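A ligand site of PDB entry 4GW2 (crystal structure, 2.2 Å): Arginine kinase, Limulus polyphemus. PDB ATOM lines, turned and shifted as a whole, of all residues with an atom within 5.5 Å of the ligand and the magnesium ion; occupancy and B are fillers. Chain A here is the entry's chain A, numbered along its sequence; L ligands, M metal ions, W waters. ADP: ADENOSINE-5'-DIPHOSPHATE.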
ATOM      1  N   SER A 122      -1.369  25.245  24.163  1.00  0.00           N
ATOM      2  CA  SER A 122      -0.324  24.524  24.895  1.00  0.00           C
ATOM      3  C   SER A 122       0.338  25.414  25.939  1.00  0.00           C
ATOM      4  O   SER A 122       0.319  26.643  25.842  1.00  0.00           O
ATOM      5  CB  SER A 122       0.732  23.986  23.938  1.00  0.00           C
ATOM      6  OG  SER A 122       1.230  25.013  23.111  1.00  0.00           O
ATOM      7  N   THR A 123       0.941  24.779  26.941  1.00  0.00           N
ATOM      8  CA  THR A 123       1.565  25.507  28.032  1.00  0.00           C
ATOM      9  C   THR A 123       2.995  25.034  28.237  1.00  0.00           C
ATOM     10  O   THR A 123       3.293  23.851  28.098  1.00  0.00           O
ATOM     11  CB  THR A 123       0.784  25.268  29.335  1.00  0.00           C
ATOM     12  OG1 THR A 123      -0.564  25.710  29.164  1.00  0.00           O
ATOM     13  CG2 THR A 123       1.430  26.018  30.491  1.00  0.00           C
ATOM     14  N   ARG A 124       3.874  25.972  28.570  1.00  0.00           N
ATOM     15  CA  ARG A 124       5.308  25.670  28.651  1.00  0.00           C
ATOM     16  C   ARG A 124       5.948  26.489  29.754  1.00  0.00           C
ATOM     17  O   ARG A 124       5.672  27.680  29.901  1.00  0.00           O
ATOM     18  CB  ARG A 124       5.946  25.979  27.301  1.00  0.00           C
ATOM     19  CG  ARG A 124       7.461  25.787  27.205  1.00  0.00           C
ATOM     20  CD  ARG A 124       7.860  25.979  25.732  1.00  0.00           C
ATOM     21  NE  ARG A 124       9.268  25.756  25.428  1.00  0.00           N
ATOM     22  CZ  ARG A 124      10.199  26.707  25.437  1.00  0.00           C
ATOM     23  NH1 ARG A 124       9.892  27.941  25.805  1.00  0.00           N
ATOM     24  NH2 ARG A 124      11.436  26.437  25.043  1.00  0.00           N
ATOM     25  N   ARG A 126      10.007  27.154  31.171  1.00  0.00           N
ATOM     26  CA  ARG A 126      11.437  26.855  31.103  1.00  0.00           C
ATOM     27  C   ARG A 126      12.260  27.595  32.140  1.00  0.00           C
ATOM     28  O   ARG A 126      11.866  28.659  32.632  1.00  0.00           O
ATOM     29  CB  ARG A 126      11.986  27.059  29.675  1.00  0.00           C
ATOM     30  CG  ARG A 126      11.969  28.473  29.122  1.00  0.00           C
ATOM     31  CD  ARG A 126      13.145  29.326  29.616  1.00  0.00           C
ATOM     32  NE  ARG A 126      13.310  30.537  28.819  1.00  0.00           N
ATOM     33  CZ  ARG A 126      13.936  31.641  29.209  1.00  0.00           C
ATOM     34  NH1 ARG A 126      14.046  32.664  28.365  1.00  0.00           N
ATOM     35  NH2 ARG A 126      14.417  31.757  30.432  1.00  0.00           N
ATOM     36  N   ILE A 182      11.986  21.425  15.405  1.00  0.00           N
ATOM     37  CA  ILE A 182      11.898  22.879  15.505  1.00  0.00           C
ATOM     38  C   ILE A 182      10.489  23.352  15.166  1.00  0.00           C
ATOM     39  O   ILE A 182       9.915  24.182  15.869  1.00  0.00           O
ATOM     40  CB  ILE A 182      12.897  23.597  14.580  1.00  0.00           C
ATOM     41  CG1 ILE A 182      14.334  23.353  15.039  1.00  0.00           C
ATOM     42  CG2 ILE A 182      12.605  25.088  14.546  1.00  0.00           C
ATOM     43  CD1 ILE A 182      15.381  23.732  14.002  1.00  0.00           C
ATOM     44  N   ASP A 184       7.754  21.734  15.447  1.00  0.00           N
ATOM     45  CA  ASP A 184       6.826  21.319  16.498  1.00  0.00           C
ATOM     46  C   ASP A 184       7.085  22.014  17.831  1.00  0.00           C
ATOM     47  O   ASP A 184       6.485  21.672  18.853  1.00  0.00           O
ATOM     48  CB  ASP A 184       6.845  19.793  16.690  1.00  0.00           C
ATOM     49  CG  ASP A 184       6.245  19.048  15.513  1.00  0.00           C
ATOM     50  OD1 ASP A 184       5.465  19.658  14.749  1.00  0.00           O
ATOM     51  OD2 ASP A 184       6.531  17.838  15.359  1.00  0.00           O
ATOM     52  N   HIS A 185       8.010  22.972  17.826  1.00  0.00           N
ATOM     53  CA  HIS A 185       8.241  23.852  18.964  1.00  0.00           C
ATOM     54  C   HIS A 185       9.035  23.194  20.101  1.00  0.00           C
ATOM     55  O   HIS A 185       9.015  23.688  21.229  1.00  0.00           O
ATOM     56  CB  HIS A 185       6.915  24.399  19.509  1.00  0.00           C
ATOM     57  CG  HIS A 185       6.026  24.995  18.459  1.00  0.00           C
ATOM     58  ND1 HIS A 185       6.424  26.045  17.668  1.00  0.00           N
ATOM     59  CD2 HIS A 185       4.774  24.672  18.067  1.00  0.00           C
ATOM     60  CE1 HIS A 185       5.449  26.348  16.834  1.00  0.00           C
ATOM     61  NE2 HIS A 185       4.438  25.534  17.059  1.00  0.00           N
ATOM     62  N   PHE A 186       9.729  22.106  19.795  1.00  0.00           N
ATOM     63  CA  PHE A 186      10.524  21.397  20.802  1.00  0.00           C
ATOM     64  C   PHE A 186      12.008  21.781  20.817  1.00  0.00           C
ATOM     65  O   PHE A 186      12.594  21.973  21.883  1.00  0.00           O
ATOM     66  CB  PHE A 186      10.409  19.878  20.604  1.00  0.00           C
ATOM     67  CG  PHE A 186       9.016  19.347  20.786  1.00  0.00           C
ATOM     68  CD1 PHE A 186       8.426  18.559  19.819  1.00  0.00           C
ATOM     69  CD2 PHE A 186       8.294  19.646  21.923  1.00  0.00           C
ATOM     70  CE1 PHE A 186       7.143  18.073  19.983  1.00  0.00           C
ATOM     71  CE2 PHE A 186       7.013  19.176  22.102  1.00  0.00           C
ATOM     72  CZ  PHE A 186       6.437  18.376  21.121  1.00  0.00           C
ATOM     73  N   LEU A 187      12.608  21.880  19.639  1.00  0.00           N
ATOM     74  CA  LEU A 187      14.044  22.101  19.559  1.00  0.00           C
ATOM     75  C   LEU A 187      14.330  23.565  19.224  1.00  0.00           C
ATOM     76  O   LEU A 187      13.583  24.209  18.498  1.00  0.00           O
ATOM     77  CB  LEU A 187      14.644  21.215  18.457  1.00  0.00           C
ATOM     78  CG  LEU A 187      16.131  21.355  18.153  1.00  0.00           C
ATOM     79  CD1 LEU A 187      16.952  21.014  19.380  1.00  0.00           C
ATOM     80  CD2 LEU A 187      16.516  20.461  16.991  1.00  0.00           C
ATOM     81  N   TRP A 221      17.672  21.546  26.553  1.00  0.00           N
ATOM     82  CA  TRP A 221      18.552  22.025  25.506  1.00  0.00           C
ATOM     83  C   TRP A 221      19.966  22.118  26.035  1.00  0.00           C
ATOM     84  O   TRP A 221      20.208  22.661  27.111  1.00  0.00           O
ATOM     85  CB  TRP A 221      18.150  23.433  25.069  1.00  0.00           C
ATOM     86  CG  TRP A 221      16.857  23.551  24.341  1.00  0.00           C
ATOM     87  CD1 TRP A 221      16.073  22.531  23.890  1.00  0.00           C
ATOM     88  CD2 TRP A 221      16.197  24.769  23.961  1.00  0.00           C
ATOM     89  NE1 TRP A 221      14.957  23.039  23.258  1.00  0.00           N
ATOM     90  CE2 TRP A 221      15.011  24.414  23.291  1.00  0.00           C
ATOM     91  CE3 TRP A 221      16.500  26.125  24.116  1.00  0.00           C
ATOM     92  CZ2 TRP A 221      14.133  25.361  22.780  1.00  0.00           C
ATOM     93  CZ3 TRP A 221      15.622  27.071  23.618  1.00  0.00           C
ATOM     94  CH2 TRP A 221      14.448  26.685  22.947  1.00  0.00           C
ATOM     95  N   GLU A 224      22.729  25.864  23.649  1.00  0.00           N
ATOM     96  CA  GLU A 224      22.216  26.938  22.809  1.00  0.00           C
ATOM     97  C   GLU A 224      22.582  28.279  23.445  1.00  0.00           C
ATOM     98  O   GLU A 224      23.765  28.553  23.642  1.00  0.00           O
ATOM     99  CB  GLU A 224      20.708  26.790  22.523  1.00  0.00           C
ATOM    100  CG  GLU A 224      20.177  27.769  21.472  1.00  0.00           C
ATOM    101  CD  GLU A 224      19.003  28.614  21.957  1.00  0.00           C
ATOM    102  OE1 GLU A 224      18.935  28.906  23.164  1.00  0.00           O
ATOM    103  OE2 GLU A 224      18.154  28.964  21.120  1.00  0.00           O
ATOM    104  N   GLU A 225      21.594  29.094  23.803  1.00  0.00           N
ATOM    105  CA  GLU A 225      21.874  30.404  24.380  1.00  0.00           C
ATOM    106  C   GLU A 225      22.499  30.256  25.772  1.00  0.00           C
ATOM    107  O   GLU A 225      23.427  30.982  26.129  1.00  0.00           O
ATOM    108  CB  GLU A 225      20.602  31.253  24.454  1.00  0.00           C
ATOM    109  CG  GLU A 225      20.786  32.585  25.172  1.00  0.00           C
ATOM    110  CD  GLU A 225      19.552  33.467  25.107  1.00  0.00           C
ATOM    111  OE1 GLU A 225      19.374  34.300  26.026  1.00  0.00           O
ATOM    112  OE2 GLU A 225      18.776  33.359  24.137  1.00  0.00           O
ATOM    113  N   ARG A 229      18.916  24.712  29.063  1.00  0.00           N
ATOM    114  CA  ARG A 229      17.550  25.175  29.269  1.00  0.00           C
ATOM    115  C   ARG A 229      16.732  23.948  29.606  1.00  0.00           C
ATOM    116  O   ARG A 229      16.768  22.954  28.881  1.00  0.00           O
ATOM    117  CB  ARG A 229      16.985  25.849  28.014  1.00  0.00           C
ATOM    118  CG  ARG A 229      17.660  27.175  27.625  1.00  0.00           C
ATOM    119  CD  ARG A 229      17.329  28.281  28.630  1.00  0.00           C
ATOM    120  NE  ARG A 229      17.805  29.601  28.210  1.00  0.00           N
ATOM    121  CZ  ARG A 229      17.262  30.342  27.251  1.00  0.00           C
ATOM    122  NH1 ARG A 229      16.178  29.918  26.613  1.00  0.00           N
ATOM    123  NH2 ARG A 229      17.788  31.520  26.943  1.00  0.00           N
ATOM    124  N   MET A 233       6.612  20.982  29.021  1.00  0.00           N
ATOM    125  CA  MET A 233       5.546  21.496  28.177  1.00  0.00           C
ATOM    126  C   MET A 233       4.593  20.382  27.748  1.00  0.00           C
ATOM    127  O   MET A 233       4.973  19.224  27.675  1.00  0.00           O
ATOM    128  CB  MET A 233       6.122  22.187  26.935  1.00  0.00           C
ATOM    129  CG  MET A 233       7.030  21.296  26.083  1.00  0.00           C
ATOM    130  SD  MET A 233       7.956  22.231  24.837  1.00  0.00           S
ATOM    131  CE  MET A 233       6.666  22.610  23.657  1.00  0.00           C
ATOM    132  N   ARG A 280      10.650  31.418  32.275  1.00  0.00           N
ATOM    133  CA  ARG A 280       9.690  31.949  31.313  1.00  0.00           C
ATOM    134  C   ARG A 280       8.552  30.960  31.151  1.00  0.00           C
ATOM    135  O   ARG A 280       8.713  29.888  30.557  1.00  0.00           O
ATOM    136  CB  ARG A 280      10.338  32.268  29.964  1.00  0.00           C
ATOM    137  CG  ARG A 280       9.442  33.114  29.042  1.00  0.00           C
ATOM    138  CD  ARG A 280      10.185  33.618  27.797  1.00  0.00           C
ATOM    139  NE  ARG A 280      10.135  32.684  26.671  1.00  0.00           N
ATOM    140  CZ  ARG A 280       9.093  32.563  25.854  1.00  0.00           C
ATOM    141  NH1 ARG A 280       8.013  33.302  26.051  1.00  0.00           N
ATOM    142  NH2 ARG A 280       9.135  31.720  24.826  1.00  0.00           N
ATOM    143  N   SER A 282       4.901  30.329  29.584  1.00  0.00           N
ATOM    144  CA  SER A 282       4.190  30.871  28.441  1.00  0.00           C
ATOM    145  C   SER A 282       3.033  29.976  28.029  1.00  0.00           C
ATOM    146  O   SER A 282       2.976  28.799  28.398  1.00  0.00           O
ATOM    147  CB  SER A 282       5.140  30.993  27.239  1.00  0.00           C
ATOM    148  OG  SER A 282       5.553  29.713  26.805  1.00  0.00           O
ATOM    149  N   VAL A 283       2.094  30.576  27.305  1.00  0.00           N
ATOM    150  CA  VAL A 283       1.084  29.825  26.599  1.00  0.00           C
ATOM    151  C   VAL A 283       1.134  30.142  25.110  1.00  0.00           C
ATOM    152  O   VAL A 283       1.521  31.235  24.704  1.00  0.00           O
ATOM    153  CB  VAL A 283      -0.323  30.139  27.129  1.00  0.00           C
ATOM    154  CG1 VAL A 283      -0.496  29.593  28.533  1.00  0.00           C
ATOM    155  CG2 VAL A 283      -0.577  31.641  27.117  1.00  0.00           C
ATOM    156  N   HIS A 284       0.737  29.172  24.297  1.00  0.00           N
ATOM    157  CA  HIS A 284       0.327  29.476  22.937  1.00  0.00           C
ATOM    158  C   HIS A 284      -1.192  29.608  22.966  1.00  0.00           C
ATOM    159  O   HIS A 284      -1.896  28.662  23.321  1.00  0.00           O
ATOM    160  CB  HIS A 284       0.718  28.359  21.982  1.00  0.00           C
ATOM    161  CG  HIS A 284       2.096  28.512  21.416  1.00  0.00           C
ATOM    162  ND1 HIS A 284       2.535  27.806  20.315  1.00  0.00           N
ATOM    163  CD2 HIS A 284       3.133  29.310  21.778  1.00  0.00           C
ATOM    164  CE1 HIS A 284       3.776  28.165  20.030  1.00  0.00           C
ATOM    165  NE2 HIS A 284       4.156  29.069  20.909  1.00  0.00           N
ATOM    166  N   ARG A 309       5.155  37.274  21.982  1.00  0.00           N
ATOM    167  CA  ARG A 309       6.071  36.795  20.956  1.00  0.00           C
ATOM    168  C   ARG A 309       5.283  36.066  19.864  1.00  0.00           C
ATOM    169  O   ARG A 309       4.152  35.666  20.077  1.00  0.00           O
ATOM    170  CB  ARG A 309       7.089  35.846  21.568  1.00  0.00           C
ATOM    171  CG  ARG A 309       8.006  36.499  22.572  1.00  0.00           C
ATOM    172  CD  ARG A 309       8.902  35.475  23.242  1.00  0.00           C
ATOM    173  NE  ARG A 309       9.772  36.107  24.223  1.00  0.00           N
ATOM    174  CZ  ARG A 309      10.977  35.650  24.575  1.00  0.00           C
ATOM    175  NH1 ARG A 309      11.437  34.526  24.052  1.00  0.00           N
ATOM    176  NH2 ARG A 309      11.690  36.308  25.478  1.00  0.00           N
ATOM    177  N   GLY A 310       5.925  35.872  18.711  1.00  0.00           N
ATOM    178  CA  GLY A 310       5.309  35.136  17.619  1.00  0.00           C
ATOM    179  C   GLY A 310       5.292  33.641  17.856  1.00  0.00           C
ATOM    180  O   GLY A 310       5.829  33.155  18.859  1.00  0.00           O
ATOM    181  N   THR A 311       4.686  32.893  16.941  1.00  0.00           N
ATOM    182  CA  THR A 311       4.492  31.460  17.130  1.00  0.00           C
ATOM    183  C   THR A 311       5.789  30.650  17.137  1.00  0.00           C
ATOM    184  O   THR A 311       5.877  29.626  17.827  1.00  0.00           O
ATOM    185  CB  THR A 311       3.548  30.886  16.053  1.00  0.00           C
ATOM    186  OG1 THR A 311       2.444  31.781  15.855  1.00  0.00           O
ATOM    187  CG2 THR A 311       3.014  29.532  16.491  1.00  0.00           C
ATOM    188  N   ARG A 312       6.785  31.106  16.394  1.00  0.00           N
ATOM    189  CA  ARG A 312       8.065  30.413  16.322  1.00  0.00           C
ATOM    190  C   ARG A 312       9.102  31.005  17.288  1.00  0.00           C
ATOM    191  O   ARG A 312      10.280  30.670  17.230  1.00  0.00           O
ATOM    192  CB  ARG A 312       8.596  30.422  14.883  1.00  0.00           C
ATOM    193  CG  ARG A 312       7.739  29.613  13.913  1.00  0.00           C
ATOM    194  CD  ARG A 312       8.242  29.695  12.484  1.00  0.00           C
ATOM    195  NE  ARG A 312       7.555  28.739  11.620  1.00  0.00           N
ATOM    196  CZ  ARG A 312       7.992  27.522  11.332  1.00  0.00           C
ATOM    197  NH1 ARG A 312       9.148  27.093  11.820  1.00  0.00           N
ATOM    198  NH2 ARG A 312       7.272  26.718  10.555  1.00  0.00           N
ATOM    199  N   GLY A 313       8.631  31.863  18.178  1.00  0.00           N
ATOM    200  CA  GLY A 313       9.461  32.450  19.213  1.00  0.00           C
ATOM    201  C   GLY A 313       9.611  33.950  19.063  1.00  0.00           C
ATOM    202  O   GLY A 313       8.951  34.560  18.222  1.00  0.00           O
ATOM    203  N   GLU A 314      10.485  34.552  19.858  1.00  0.00           N
ATOM    204  CA  GLU A 314      10.754  35.986  19.769  1.00  0.00           C
ATOM    205  C   GLU A 314      11.181  36.381  18.351  1.00  0.00           C
ATOM    206  O   GLU A 314      11.801  35.584  17.651  1.00  0.00           O
ATOM    207  CB  GLU A 314      11.805  36.385  20.795  1.00  0.00           C
ATOM    208  CG  GLU A 314      13.096  35.587  20.702  1.00  0.00           C
ATOM    209  CD  GLU A 314      14.202  36.170  21.562  1.00  0.00           C
ATOM    210  OE1 GLU A 314      13.930  37.132  22.297  1.00  0.00           O
ATOM    211  OE2 GLU A 314      15.331  35.636  21.527  1.00  0.00           O
ATOM    212  N   ASP A 324       2.453  33.712  21.418  1.00  0.00           N
ATOM    213  CA  ASP A 324       3.173  33.265  22.602  1.00  0.00           C
ATOM    214  C   ASP A 324       3.122  34.389  23.632  1.00  0.00           C
ATOM    215  O   ASP A 324       3.667  35.466  23.404  1.00  0.00           O
ATOM    216  CB  ASP A 324       4.619  32.955  22.208  1.00  0.00           C
ATOM    217  CG  ASP A 324       5.541  32.754  23.402  1.00  0.00           C
ATOM    218  OD1 ASP A 324       5.236  33.237  24.504  1.00  0.00           O
ATOM    219  OD2 ASP A 324       6.605  32.128  23.211  1.00  0.00           O
HETATM  220  PB  ADP L   1      12.990  30.601  25.044  1.00  0.00           P
HETATM  221  O1B ADP L   1      14.362  30.866  24.478  1.00  0.00           O
HETATM  222  O2B ADP L   1      12.518  29.162  25.010  1.00  0.00           O
HETATM  223  O3B ADP L   1      12.714  31.417  26.280  1.00  0.00           O
HETATM  224  PA  ADP L   1      11.987  31.522  22.376  1.00  0.00           P
HETATM  225  O1A ADP L   1      13.344  31.406  21.766  1.00  0.00           O
HETATM  226  O2A ADP L   1      10.947  32.459  21.813  1.00  0.00           O
HETATM  227  O3A ADP L   1      11.785  31.030  23.818  1.00  0.00           O
HETATM  228  O5' ADP L   1      11.327  30.054  21.510  1.00  0.00           O
HETATM  229  C5' ADP L   1      11.774  28.821  21.767  1.00  0.00           C
HETATM  230  C4' ADP L   1      10.768  27.714  21.231  1.00  0.00           C
HETATM  231  O4' ADP L   1       9.721  27.514  22.193  1.00  0.00           O
HETATM  232  C3' ADP L   1      10.042  28.144  19.939  1.00  0.00           C
HETATM  233  O3' ADP L   1       9.889  27.087  19.053  1.00  0.00           O
HETATM  234  C2' ADP L   1       8.603  28.501  20.421  1.00  0.00           C
HETATM  235  O2' ADP L   1       7.638  28.101  19.503  1.00  0.00           O
HETATM  236  C1' ADP L   1       8.503  27.487  21.564  1.00  0.00           C
HETATM  237  N9  ADP L   1       7.406  27.761  22.540  1.00  0.00           N
HETATM  238  C8  ADP L   1       7.375  28.854  23.441  1.00  0.00           C
HETATM  239  N7  ADP L   1       6.279  28.860  24.211  1.00  0.00           N
HETATM  240  C5  ADP L   1       5.558  27.729  23.803  1.00  0.00           C
HETATM  241  C6  ADP L   1       4.323  27.180  24.219  1.00  0.00           C
HETATM  242  N6  ADP L   1       3.584  27.776  25.218  1.00  0.00           N
HETATM  243  N1  ADP L   1       3.827  26.035  23.636  1.00  0.00           N
HETATM  244  C2  ADP L   1       4.597  25.486  22.654  1.00  0.00           C
HETATM  245  N3  ADP L   1       5.787  25.888  22.158  1.00  0.00           N
HETATM  246  C4  ADP L   1       6.246  27.038  22.763  1.00  0.00           C
HETATM  247 MG    MG M   1      15.448  31.218  22.759  1.00  0.00          MG
HETATM  248  O   HOH W   1      11.136  28.213  16.142  1.00  0.00           O
HETATM  249  O   HOH W   2       6.523  30.953  20.640  1.00  0.00           O
HETATM  250  O   HOH W   3       8.954  26.416  16.560  1.00  0.00           O
HETATM  251  O   HOH W   4      12.559  26.962  18.291  1.00  0.00           O
HETATM  252  O   HOH W   5      14.660  33.063  23.209  1.00  0.00           O
HETATM  253  O   HOH W   6      17.307  31.257  23.643  1.00  0.00           O
HETATM  254  O   HOH W   7      13.964  31.367  19.085  1.00  0.00           O
HETATM  255  O   HOH W   8      15.897  32.368  21.061  1.00  0.00           O
HETATM  256  O   HOH W   9      15.477  29.630  21.432  1.00  0.00           O
HETATM  257  O   HOH W  10      14.442  27.534  26.660  1.00  0.00           O
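The magnesium ion is bound by water W5 (2.1 Å), water W6 (2.1 Å), O1B of the ligand (2.1 Å), water W9 (2.1 Å), water W8 (2.1 Å) and O1A of the ligand (2.3 Å). The magnesium ion has six donor atoms within binding distance.
Glu 224 touches the magnesium ion. Of the 25 residues printed, 1 comes within 4 Å of the magnesium ion.
A nitrogen (N6) of the ligand lies close to the backbone NH (N) of His 284, 3.3 Å away. A nitrogen (N7) of the ligand lies close to the side-chain carboxylate (OD2) of Asp 324 (3.4 Å). Trp 221 touches the ligand (CH2 to C5', 3.6 Å). Met 233 touches the ligand (CE to C2, 3.7 Å). C of Val 283 touches N6 of the ligand, at 3.4 Å. O of Arg 312 touches C3' of the ligand, at 3.7 Å. Gly 313 touches the ligand (CA to O2A, 3.0 Å). Hydrophobic or aromatic side chains that line the ligand: His 185, Trp 221, Met 233 and His 284. Of the 25 residues printed, 17 come within 4 Å of the ligand. The nearest printed residue that does not touch the ligand is Thr 123 (4.1 Å).
NE of Arg 280 is in salt-bridge range of O3B of the ligand (2.9 Å). N1 of the ligand lies within hydrogen-bond range of OG of Ser 122. The side-chain hydroxyl (OG) of Ser 282 sits at hydrogen-bond distance from a nitrogen (N7) of the ligand. The guanidinium group (NE) of Arg 126 is in salt-bridge range of an oxygen (O3B) of the ligand (2.8 Å). NH1 of Arg 309 is in salt-bridge range of O2A of the ligand, at 3.1 Å. N of Glu 314 lies within hydrogen-bond range of O2A of the ligand (2.9 Å). An oxygen (O2') of the ligand is in hydrogen-bond range of the backbone carbonyl oxygen (O) of Thr 311 (2.9 Å). The backbone carbonyl oxygen (O) of Ser 282 is in hydrogen-bond range of a nitrogen (N6) of the ligand. A ring nitrogen (ND1) of His 185 is in hydrogen-bond range of an oxygen (O2') of the ligand, 3.0 Å away. NH1 of Arg 229 lies within salt-bridge range of O3B of the ligand (3.8 Å). An oxygen (O2B) of the ligand lies within salt-bridge range of the guanidinium group (NH2) of Arg 124, 2.9 Å away.
Water W6 lies within hydrogen-bond range of OE2 of Glu 225 (2.6 Å), OE1 of Glu 224 (2.9 Å) and NH2 of Arg 229 (3.3 Å). Water W3 lies within hydrogen-bond range of the backbone carbonyl oxygen of Ile 182, an oxygen (O3') of the ligand and a ring nitrogen (ND1) of His 185. Water W4 bridges an oxygen (O3') of the ligand (2.8 Å) and the backbone carbonyl oxygen (O) of Leu 187 (2.9 Å). Water W10 lies within hydrogen-bond range of the guanidinium group (NH1) of Arg 229 (2.9 Å) and an oxygen (O2B) of the ligand (3.0 Å). Water W1 bridges O of Arg 312 (2.8 Å) and O3' of the ligand (3.4 Å).
The backbone carbonyl oxygen (O) of Arg 126 is in hydrogen-bond range of the backbone NH (N) of Arg 280 (3.0 Å). The backbone NH of Arg 309 sits at hydrogen-bond distance from the backbone carbonyl oxygen of Asp 324, 2.7 Å away. O of Ser 122 sits at hydrogen-bond distance from N of His 284, 3.0 Å away. N of Ser 282 is in hydrogen-bond range of O of Arg 124 (2.8 Å). OE1 of Glu 314 lies within salt-bridge range of NH2 of Arg 309. The guanidinium group (NH2) of Arg 280 lies within salt-bridge range of the side-chain carboxylate (OD2) of Asp 324 (3.0 Å). OE1 of Glu 225 lies within salt-bridge range of NH2 of Arg 229, at 3.3 Å. NE1 of Trp 221 is in hydrogen-bond range of O of Phe 186, at 2.9 Å.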
